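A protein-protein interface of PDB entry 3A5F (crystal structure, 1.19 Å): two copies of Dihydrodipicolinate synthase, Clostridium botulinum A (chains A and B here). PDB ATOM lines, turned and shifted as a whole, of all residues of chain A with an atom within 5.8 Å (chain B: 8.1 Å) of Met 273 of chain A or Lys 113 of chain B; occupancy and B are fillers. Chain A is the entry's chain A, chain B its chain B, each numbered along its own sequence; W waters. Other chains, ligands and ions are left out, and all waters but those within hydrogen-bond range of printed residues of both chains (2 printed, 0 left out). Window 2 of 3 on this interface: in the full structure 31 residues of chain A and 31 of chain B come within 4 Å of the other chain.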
ATOM      1  N   ALA A 242     -12.397  -4.028  17.523  1.00  0.00           N
ATOM      2  CA  ALA A 242     -11.908  -5.407  17.315  1.00  0.00           C
ATOM      3  C   ALA A 242     -11.979  -5.820  15.851  1.00  0.00           C
ATOM      4  O   ALA A 242     -11.143  -6.591  15.392  1.00  0.00           O
ATOM      5  CB  ALA A 242     -12.601  -6.405  18.230  1.00  0.00           C
ATOM      6  N   ILE A 245      -8.741  -4.783  14.284  1.00  0.00           N
ATOM      7  CA  ILE A 245      -7.508  -5.091  14.973  1.00  0.00           C
ATOM      8  C   ILE A 245      -6.484  -5.649  14.007  1.00  0.00           C
ATOM      9  O   ILE A 245      -5.275  -5.543  14.258  1.00  0.00           O
ATOM     10  CB  ILE A 245      -7.791  -6.055  16.124  1.00  0.00           C
ATOM     11  CG1 ILE A 245      -6.651  -6.131  17.150  1.00  0.00           C
ATOM     12  CG2 ILE A 245      -8.131  -7.468  15.674  1.00  0.00           C
ATOM     13  CD1 ILE A 245      -7.057  -6.849  18.458  1.00  0.00           C
ATOM     14  N   GLU A 246      -6.944  -6.270  12.933  1.00  0.00           N
ATOM     15  CA  GLU A 246      -6.184  -6.661  11.755  1.00  0.00           C
ATOM     16  C   GLU A 246      -6.911  -6.105  10.574  1.00  0.00           C
ATOM     17  O   GLU A 246      -8.093  -5.801  10.653  1.00  0.00           O
ATOM     18  CB  GLU A 246      -6.072  -8.192  11.644  1.00  0.00           C
ATOM     19  CG  GLU A 246      -5.285  -8.788  12.827  1.00  0.00           C
ATOM     20  CD  GLU A 246      -4.823 -10.188  12.712  1.00  0.00           C
ATOM     21  OE1 GLU A 246      -5.121 -10.797  11.615  1.00  0.00           O
ATOM     22  OE2 GLU A 246      -4.198 -10.761  13.677  1.00  0.00           O
ATOM     23  N   ILE A 250     -10.261  -9.307   7.470  1.00  0.00           N
ATOM     24  CA  ILE A 250      -9.832 -10.409   8.255  1.00  0.00           C
ATOM     25  C   ILE A 250     -10.692 -10.613   9.486  1.00  0.00           C
ATOM     26  O   ILE A 250     -11.254 -11.700   9.679  1.00  0.00           O
ATOM     27  CB  ILE A 250      -8.332 -10.391   8.539  1.00  0.00           C
ATOM     28  CG1 ILE A 250      -7.492 -10.539   7.264  1.00  0.00           C
ATOM     29  CG2 ILE A 250      -7.995 -11.472   9.562  1.00  0.00           C
ATOM     30  CD1 ILE A 250      -6.012 -10.216   7.473  1.00  0.00           C
ATOM     31  N   PRO A 251     -10.872  -9.591  10.329  1.00  0.00           N
ATOM     32  CA  PRO A 251     -11.680  -9.840  11.500  1.00  0.00           C
ATOM     33  C   PRO A 251     -13.112 -10.095  11.231  1.00  0.00           C
ATOM     34  O   PRO A 251     -13.723 -10.955  11.881  1.00  0.00           O
ATOM     35  CB  PRO A 251     -11.502  -8.558  12.356  1.00  0.00           C
ATOM     36  CG  PRO A 251     -10.143  -8.041  11.891  1.00  0.00           C
ATOM     37  CD  PRO A 251     -10.168  -8.308  10.407  1.00  0.00           C
ATOM     38  N   THR A 254     -13.686 -13.616  10.090  1.00  0.00           N
ATOM     39  CA  THR A 254     -13.430 -14.468  11.223  1.00  0.00           C
ATOM     40  C   THR A 254     -14.607 -14.483  12.167  1.00  0.00           C
ATOM     41  O   THR A 254     -15.039 -15.516  12.668  1.00  0.00           O
ATOM     42  CB  THR A 254     -12.125 -14.057  11.928  1.00  0.00           C
ATOM     43  OG1 THR A 254     -11.057 -14.083  10.978  1.00  0.00           O
ATOM     44  CG2 THR A 254     -11.790 -14.880  13.141  1.00  0.00           C
ATOM     45  N   CYS A 271      -5.220 -13.481   5.530  1.00  0.00           N
ATOM     46  CA  CYS A 271      -5.031 -14.754   6.175  1.00  0.00           C
ATOM     47  C   CYS A 271      -5.631 -14.716   7.545  1.00  0.00           C
ATOM     48  O   CYS A 271      -6.096 -13.682   8.020  1.00  0.00           O
ATOM     49  CB  CYS A 271      -3.567 -15.136   6.212  1.00  0.00           C
ATOM     50  SG  CYS A 271      -2.573 -14.066   7.293  1.00  0.00           S
ATOM     51  N   GLU A 272      -5.536 -15.809   8.245  1.00  0.00           N
ATOM     52  CA  GLU A 272      -6.011 -16.019   9.571  1.00  0.00           C
ATOM     53  C   GLU A 272      -5.394 -15.045  10.553  1.00  0.00           C
ATOM     54  O   GLU A 272      -4.191 -14.700  10.454  1.00  0.00           O
ATOM     55  CB  GLU A 272      -5.650 -17.453  10.000  1.00  0.00           C
ATOM     56  CG  GLU A 272      -6.654 -18.444   9.429  1.00  0.00           C
ATOM     57  CD  GLU A 272      -6.452 -19.823   9.970  1.00  0.00           C
ATOM     58  OE1 GLU A 272      -5.508 -19.968  10.815  1.00  0.00           O
ATOM     59  OE2 GLU A 272      -7.196 -20.741   9.563  1.00  0.00           O
ATOM     60  N   MET A 273      -6.152 -14.642  11.556  1.00  0.00           N
ATOM     61  CA  MET A 273      -5.670 -13.835  12.622  1.00  0.00           C
ATOM     62  C   MET A 273      -4.612 -14.508  13.468  1.00  0.00           C
ATOM     63  O   MET A 273      -4.542 -15.741  13.572  1.00  0.00           O
ATOM     64  CB  MET A 273      -6.854 -13.432  13.539  1.00  0.00           C
ATOM     65  CG  MET A 273      -7.909 -12.635  12.877  1.00  0.00           C
ATOM     66  SD  MET A 273      -9.309 -12.111  13.767  1.00  0.00           S
ATOM     67  CE  MET A 273      -8.613 -10.965  14.849  1.00  0.00           C
ATOM     68  N   ASN A 274      -3.784 -13.708  14.154  1.00  0.00           N
ATOM     69  CA  ASN A 274      -2.885 -14.240  15.148  1.00  0.00           C
ATOM     70  C   ASN A 274      -3.648 -14.541  16.436  1.00  0.00           C
ATOM     71  O   ASN A 274      -4.823 -14.211  16.591  1.00  0.00           O
ATOM     72  CB  ASN A 274      -1.662 -13.331  15.340  1.00  0.00           C
ATOM     73  CG  ASN A 274      -1.909 -12.109  16.108  1.00  0.00           C
ATOM     74  OD1 ASN A 274      -2.847 -11.958  16.849  1.00  0.00           O
ATOM     75  ND2 ASN A 274      -0.969 -11.166  15.950  1.00  0.00           N
ATOM     76  N   GLU A 275      -2.998 -15.268  17.340  1.00  0.00           N
ATOM     77  CA  GLU A 275      -3.644 -15.737  18.537  1.00  0.00           C
ATOM     78  C   GLU A 275      -4.178 -14.645  19.409  1.00  0.00           C
ATOM     79  O   GLU A 275      -5.340 -14.715  19.904  1.00  0.00           O
ATOM     80  CB  GLU A 275      -2.737 -16.610  19.371  1.00  0.00           C
ATOM     81  CG  GLU A 275      -2.401 -17.910  18.731  1.00  0.00           C
ATOM     82  CD  GLU A 275      -1.214 -18.583  19.485  1.00  0.00           C
ATOM     83  OE1 GLU A 275      -0.874 -18.172  20.639  1.00  0.00           O
ATOM     84  OE2 GLU A 275      -0.658 -19.513  18.948  1.00  0.00           O
ATOM     85  N   ASN A 277      -4.890 -11.544  18.747  1.00  0.00           N
ATOM     86  CA  ASN A 277      -5.957 -10.773  18.189  1.00  0.00           C
ATOM     87  C   ASN A 277      -7.235 -11.544  18.084  1.00  0.00           C
ATOM     88  O   ASN A 277      -8.341 -10.996  18.253  1.00  0.00           O
ATOM     89  CB  ASN A 277      -5.514 -10.210  16.859  1.00  0.00           C
ATOM     90  CG  ASN A 277      -4.416  -9.169  16.946  1.00  0.00           C
ATOM     91  OD1 ASN A 277      -4.227  -8.564  17.979  1.00  0.00           O
ATOM     92  ND2 ASN A 277      -3.709  -8.995  15.845  1.00  0.00           N
ATOM     93  N   LEU A 278      -7.147 -12.840  17.753  1.00  0.00           N
ATOM     94  CA  LEU A 278      -8.342 -13.667  17.782  1.00  0.00           C
ATOM     95  C   LEU A 278      -9.010 -13.665  19.130  1.00  0.00           C
ATOM     96  O   LEU A 278     -10.224 -13.598  19.225  1.00  0.00           O
ATOM     97  CB  LEU A 278      -7.957 -15.071  17.349  1.00  0.00           C
ATOM     98  CG  LEU A 278      -9.094 -16.057  17.304  1.00  0.00           C
ATOM     99  CD1 LEU A 278     -10.167 -15.670  16.279  1.00  0.00           C
ATOM    100  CD2 LEU A 278      -8.594 -17.475  16.994  1.00  0.00           C
ATOM    101  N   LEU A 281     -10.945 -10.468  19.617  1.00  0.00           N
ATOM    102  CA  LEU A 281     -12.161 -10.497  18.875  1.00  0.00           C
ATOM    103  C   LEU A 281     -13.207 -11.370  19.560  1.00  0.00           C
ATOM    104  O   LEU A 281     -14.362 -11.022  19.700  1.00  0.00           O
ATOM    105  CB  LEU A 281     -11.905 -10.968  17.466  1.00  0.00           C
ATOM    106  CG  LEU A 281     -13.107 -11.097  16.551  1.00  0.00           C
ATOM    107  CD1 LEU A 281     -13.862  -9.750  16.366  1.00  0.00           C
ATOM    108  CD2 LEU A 281     -12.715 -11.712  15.244  1.00  0.00           C
ATOM    109  N   THR B 110      -2.541  -6.329   4.190  1.00  0.00           N
ATOM    110  CA  THR B 110      -2.623  -7.506   4.946  1.00  0.00           C
ATOM    111  C   THR B 110      -1.826  -7.241   6.243  1.00  0.00           C
ATOM    112  O   THR B 110      -1.308  -6.145   6.411  1.00  0.00           O
ATOM    113  CB  THR B 110      -2.123  -8.750   4.178  1.00  0.00           C
ATOM    114  OG1 THR B 110      -2.478  -9.880   5.005  1.00  0.00           O
ATOM    115  CG2 THR B 110      -0.638  -8.711   3.906  1.00  0.00           C
ATOM    116  N   THR B 111      -1.726  -8.248   7.090  1.00  0.00           N
ATOM    117  CA  THR B 111      -0.983  -8.206   8.350  1.00  0.00           C
ATOM    118  C   THR B 111       0.460  -8.566   8.069  1.00  0.00           C
ATOM    119  O   THR B 111       0.823  -9.055   6.990  1.00  0.00           O
ATOM    120  CB  THR B 111      -1.640  -9.159   9.329  1.00  0.00           C
ATOM    121  OG1 THR B 111      -1.572 -10.459   8.722  1.00  0.00           O
ATOM    122  CG2 THR B 111      -3.049  -8.735   9.647  1.00  0.00           C
ATOM    123  N   GLN B 112       1.342  -8.437   9.067  1.00  0.00           N
ATOM    124  CA  GLN B 112       2.702  -8.921   8.914  1.00  0.00           C
ATOM    125  C   GLN B 112       2.707 -10.447   8.671  1.00  0.00           C
ATOM    126  O   GLN B 112       3.466 -10.957   7.878  1.00  0.00           O
ATOM    127  CB  GLN B 112       3.592  -8.550  10.106  1.00  0.00           C
ATOM    128  CG  GLN B 112       3.750  -7.010  10.279  1.00  0.00           C
ATOM    129  CD  GLN B 112       4.395  -6.271   9.132  1.00  0.00           C
ATOM    130  OE1 GLN B 112       5.455  -6.636   8.645  1.00  0.00           O
ATOM    131  NE2 GLN B 112       3.715  -5.256   8.659  1.00  0.00           N
ATOM    132  N   LYS B 113       1.810 -11.164   9.362  1.00  0.00           N
ATOM    133  CA  LYS B 113       1.637 -12.601   9.140  1.00  0.00           C
ATOM    134  C   LYS B 113       1.279 -12.869   7.710  1.00  0.00           C
ATOM    135  O   LYS B 113       1.835 -13.778   7.064  1.00  0.00           O
ATOM    136  CB  LYS B 113       0.598 -13.136  10.107  1.00  0.00           C
ATOM    137  CG  LYS B 113       0.231 -14.550   9.983  1.00  0.00           C
ATOM    138  CD  LYS B 113      -0.760 -14.978  11.052  1.00  0.00           C
ATOM    139  CE  LYS B 113      -1.332 -16.359  10.819  1.00  0.00           C
ATOM    140  NZ  LYS B 113      -2.242 -16.793  11.874  1.00  0.00           N
ATOM    141  N   GLY B 114       0.377 -12.081   7.167  1.00  0.00           N
ATOM    142  CA  GLY B 114      -0.028 -12.242   5.786  1.00  0.00           C
ATOM    143  C   GLY B 114       1.076 -11.896   4.815  1.00  0.00           C
ATOM    144  O   GLY B 114       1.205 -12.513   3.772  1.00  0.00           O
ATOM    145  N   LEU B 115       1.936 -10.902   5.132  1.00  0.00           N
ATOM    146  CA  LEU B 115       3.051 -10.588   4.295  1.00  0.00           C
ATOM    147  C   LEU B 115       3.989 -11.754   4.160  1.00  0.00           C
ATOM    148  O   LEU B 115       4.500 -12.072   3.092  1.00  0.00           O
ATOM    149  CB  LEU B 115       3.809  -9.356   4.866  1.00  0.00           C
ATOM    150  CG  LEU B 115       3.179  -8.000   4.551  1.00  0.00           C
ATOM    151  CD1 LEU B 115       3.820  -6.914   5.412  1.00  0.00           C
ATOM    152  CD2 LEU B 115       3.247  -7.714   3.047  1.00  0.00           C
ATOM    153  N   VAL B 116       4.271 -12.440   5.271  1.00  0.00           N
ATOM    154  CA  VAL B 116       5.115 -13.639   5.205  1.00  0.00           C
ATOM    155  C   VAL B 116       4.495 -14.663   4.280  1.00  0.00           C
ATOM    156  O   VAL B 116       5.114 -15.210   3.385  1.00  0.00           O
ATOM    157  CB  VAL B 116       5.414 -14.167   6.563  1.00  0.00           C
ATOM    158  CG1 VAL B 116       6.184 -15.494   6.503  1.00  0.00           C
ATOM    159  CG2 VAL B 116       6.184 -13.190   7.421  1.00  0.00           C
ATOM    160  N   LYS B 117       3.168 -14.907   4.442  1.00  0.00           N
ATOM    161  CA  LYS B 117       2.492 -15.864   3.554  1.00  0.00           C
ATOM    162  C   LYS B 117       2.517 -15.462   2.122  1.00  0.00           C
ATOM    163  O   LYS B 117       2.738 -16.336   1.260  1.00  0.00           O
ATOM    164  CB  LYS B 117       1.060 -16.063   4.030  1.00  0.00           C
ATOM    165  CG  LYS B 117       0.976 -16.840   5.327  1.00  0.00           C
ATOM    166  CD  LYS B 117      -0.380 -16.906   5.876  1.00  0.00           C
ATOM    167  CE  LYS B 117      -0.528 -17.625   7.174  1.00  0.00           C
ATOM    168  NZ  LYS B 117      -0.221 -18.981   7.160  1.00  0.00           N
ATOM    169  N   HIS B 118       2.311 -14.183   1.837  1.00  0.00           N
ATOM    170  CA  HIS B 118       2.321 -13.701   0.473  1.00  0.00           C
ATOM    171  C   HIS B 118       3.653 -13.914  -0.203  1.00  0.00           C
ATOM    172  O   HIS B 118       3.761 -14.492  -1.270  1.00  0.00           O
ATOM    173  CB  HIS B 118       1.968 -12.234   0.451  1.00  0.00           C
ATOM    174  CG  HIS B 118       2.027 -11.557  -0.858  1.00  0.00           C
ATOM    175  ND1 HIS B 118       1.000 -11.648  -1.772  1.00  0.00           N
ATOM    176  CD2 HIS B 118       3.013 -10.794  -1.393  1.00  0.00           C
ATOM    177  CE1 HIS B 118       1.372 -10.904  -2.836  1.00  0.00           C
ATOM    178  NE2 HIS B 118       2.582 -10.438  -2.649  1.00  0.00           N
ATOM    179  N   PHE B 119       4.726 -13.486   0.468  1.00  0.00           N
ATOM    180  CA  PHE B 119       6.046 -13.592  -0.103  1.00  0.00           C
ATOM    181  C   PHE B 119       6.532 -14.998  -0.206  1.00  0.00           C
ATOM    182  O   PHE B 119       7.158 -15.388  -1.167  1.00  0.00           O
ATOM    183  CB  PHE B 119       7.049 -12.667   0.588  1.00  0.00           C
ATOM    184  CG  PHE B 119       6.864 -11.220   0.163  1.00  0.00           C
ATOM    185  CD1 PHE B 119       7.259 -10.818  -1.115  1.00  0.00           C
ATOM    186  CD2 PHE B 119       6.304 -10.308   1.010  1.00  0.00           C
ATOM    187  CE1 PHE B 119       7.049  -9.508  -1.524  1.00  0.00           C
ATOM    188  CE2 PHE B 119       6.090  -9.014   0.567  1.00  0.00           C
ATOM    189  CZ  PHE B 119       6.460  -8.632  -0.653  1.00  0.00           C
ATOM    190  N   LYS B 120       6.202 -15.819   0.777  1.00  0.00           N
ATOM    191  CA  LYS B 120       6.522 -17.217   0.682  1.00  0.00           C
ATOM    192  C   LYS B 120       5.771 -17.925  -0.422  1.00  0.00           C
ATOM    193  O   LYS B 120       6.327 -18.801  -1.092  1.00  0.00           O
ATOM    194  CB  LYS B 120       6.332 -17.927   2.036  1.00  0.00           C
ATOM    195  CG  LYS B 120       7.324 -17.548   3.094  1.00  0.00           C
ATOM    196  CD  LYS B 120       7.246 -18.365   4.369  1.00  0.00           C
ATOM    197  CE  LYS B 120       8.452 -18.072   5.342  1.00  0.00           C
ATOM    198  N   THR B 147       9.699  -8.666  10.028  1.00  0.00           N
ATOM    199  CA  THR B 147       9.124  -9.527   9.014  1.00  0.00           C
ATOM    200  C   THR B 147      10.147  -9.863   7.925  1.00  0.00           C
ATOM    201  O   THR B 147      10.203 -11.004   7.450  1.00  0.00           O
ATOM    202  CB  THR B 147       7.893  -8.856   8.384  1.00  0.00           C
ATOM    203  OG1 THR B 147       6.974  -8.721   9.457  1.00  0.00           O
ATOM    204  CG2 THR B 147       7.304  -9.641   7.232  1.00  0.00           C
ATOM    205  N   LEU B 151      11.827 -13.589   6.335  1.00  0.00           N
ATOM    206  CA  LEU B 151      11.829 -13.884   4.890  1.00  0.00           C
ATOM    207  C   LEU B 151      13.246 -14.007   4.307  1.00  0.00           C
ATOM    208  O   LEU B 151      13.380 -14.602   3.297  1.00  0.00           O
ATOM    209  CB  LEU B 151      11.046 -12.813   4.159  1.00  0.00           C
ATOM    210  CG  LEU B 151       9.532 -12.860   4.345  1.00  0.00           C
ATOM    211  CD1 LEU B 151       8.866 -11.599   3.844  1.00  0.00           C
ATOM    212  CD2 LEU B 151       8.962 -14.160   3.734  1.00  0.00           C
HETATM  213  O   HOH W   1      -2.695 -19.082  10.557  1.00  0.00           O
HETATM  214  O   HOH W   2      -3.229 -12.086  10.249  1.00  0.00           O
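Hydrophobic or aromatic side chains of chain A within 4 Å of the printed part of chain B: Ile 250.
Along chain A the printed residues that touch a printed residue of chain B span positions 246 to 273.
Among the printed residues, 7 pairs touch across the chains.
Glu 246 of chain A touches Thr 111 of chain B (OE1 to CG2, 3.5 Å).
Thr 111 of chain B touches Ile 250 of chain A (CG2 to CD1, 3.96 Å).
CG of Lys 113 of chain B touches SG of Cys 271 of chain A, at 3.9 Å.
Cys 271 of chain A touches Lys 117 of chain B.
Of the printed residues of chain B, Cys 271 of chain A touches Lys 113, Gly 114 and Lys 117.
Of chain B, only Lys 113 comes within 4 Å of Met 273 of chain A.
Asn 274 of chain A touches none of the printed residues of chain B.
Printed residues of chain A within 4 Å of Thr 111 of chain B: Glu 246 (3.5 Å) and Ile 250 (3.96 Å).
Printed residues of chain A within 4 Å of Lys 113 of chain B: Cys 271 (3.9 Å), Glu 272 (3.2 Å) and Met 273 (3.0 Å).
Of the printed residues of chain A, Lys 117 of chain B touches Cys 271 (3.7 Å).
No position is printed for both chains.
Of the 7 pairs that touch across the chains among the printed residues, none has its exchanged pair printed and touching as well.
Water W2 lies within hydrogen-bond range of the side-chain carboxylate (OE1) of Glu 246 of chain A (2.7 Å), the side-chain hydroxyl (OG1) of Thr 111 of chain B (2.8 Å), the backbone carbonyl oxygen (O) of Glu 272 of chain A (2.8 Å) and the side-chain sulfur (SG) of Cys 271 of chain A (3.6 Å).
Water W1 bridges the side-chain amino group of Lys 113 of chain B (2.7 Å) and the side-chain carboxylate of Glu 272 of chain A (3.0 Å).
The backbone NH (N) of Gly 114 of chain B sits close to the side-chain sulfur (SG) of Cys 271 of chain A.
The backbone carbonyl oxygen (O) of Met 273 of chain A sits at hydrogen-bond distance from the side-chain amino group (NZ) of Lys 113 of chain B (3.0 Å).
O of Glu 272 of chain A is in hydrogen-bond range of NZ of Lys 113 of chain B (3.2 Å).
The side-chain hydroxyl (OG1) of Thr 111 of chain B sits at hydrogen-bond distance from the backbone NH (N) of Gly 114 of chain B, at 3.0 Å.
OE2 of Glu 246 of chain A lies within hydrogen-bond range of N of Asn 274 of chain A (3.0 Å).
O of Ile 250 of chain A sits at hydrogen-bond distance from OG1 of Thr 254 of chain A, at 2.7 Å.
The side-chain carboxylate (OE2) of Glu 246 of chain A is in hydrogen-bond range of the side-chain amide nitrogen (ND2) of Asn 277 of chain A, 2.8 Å away.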
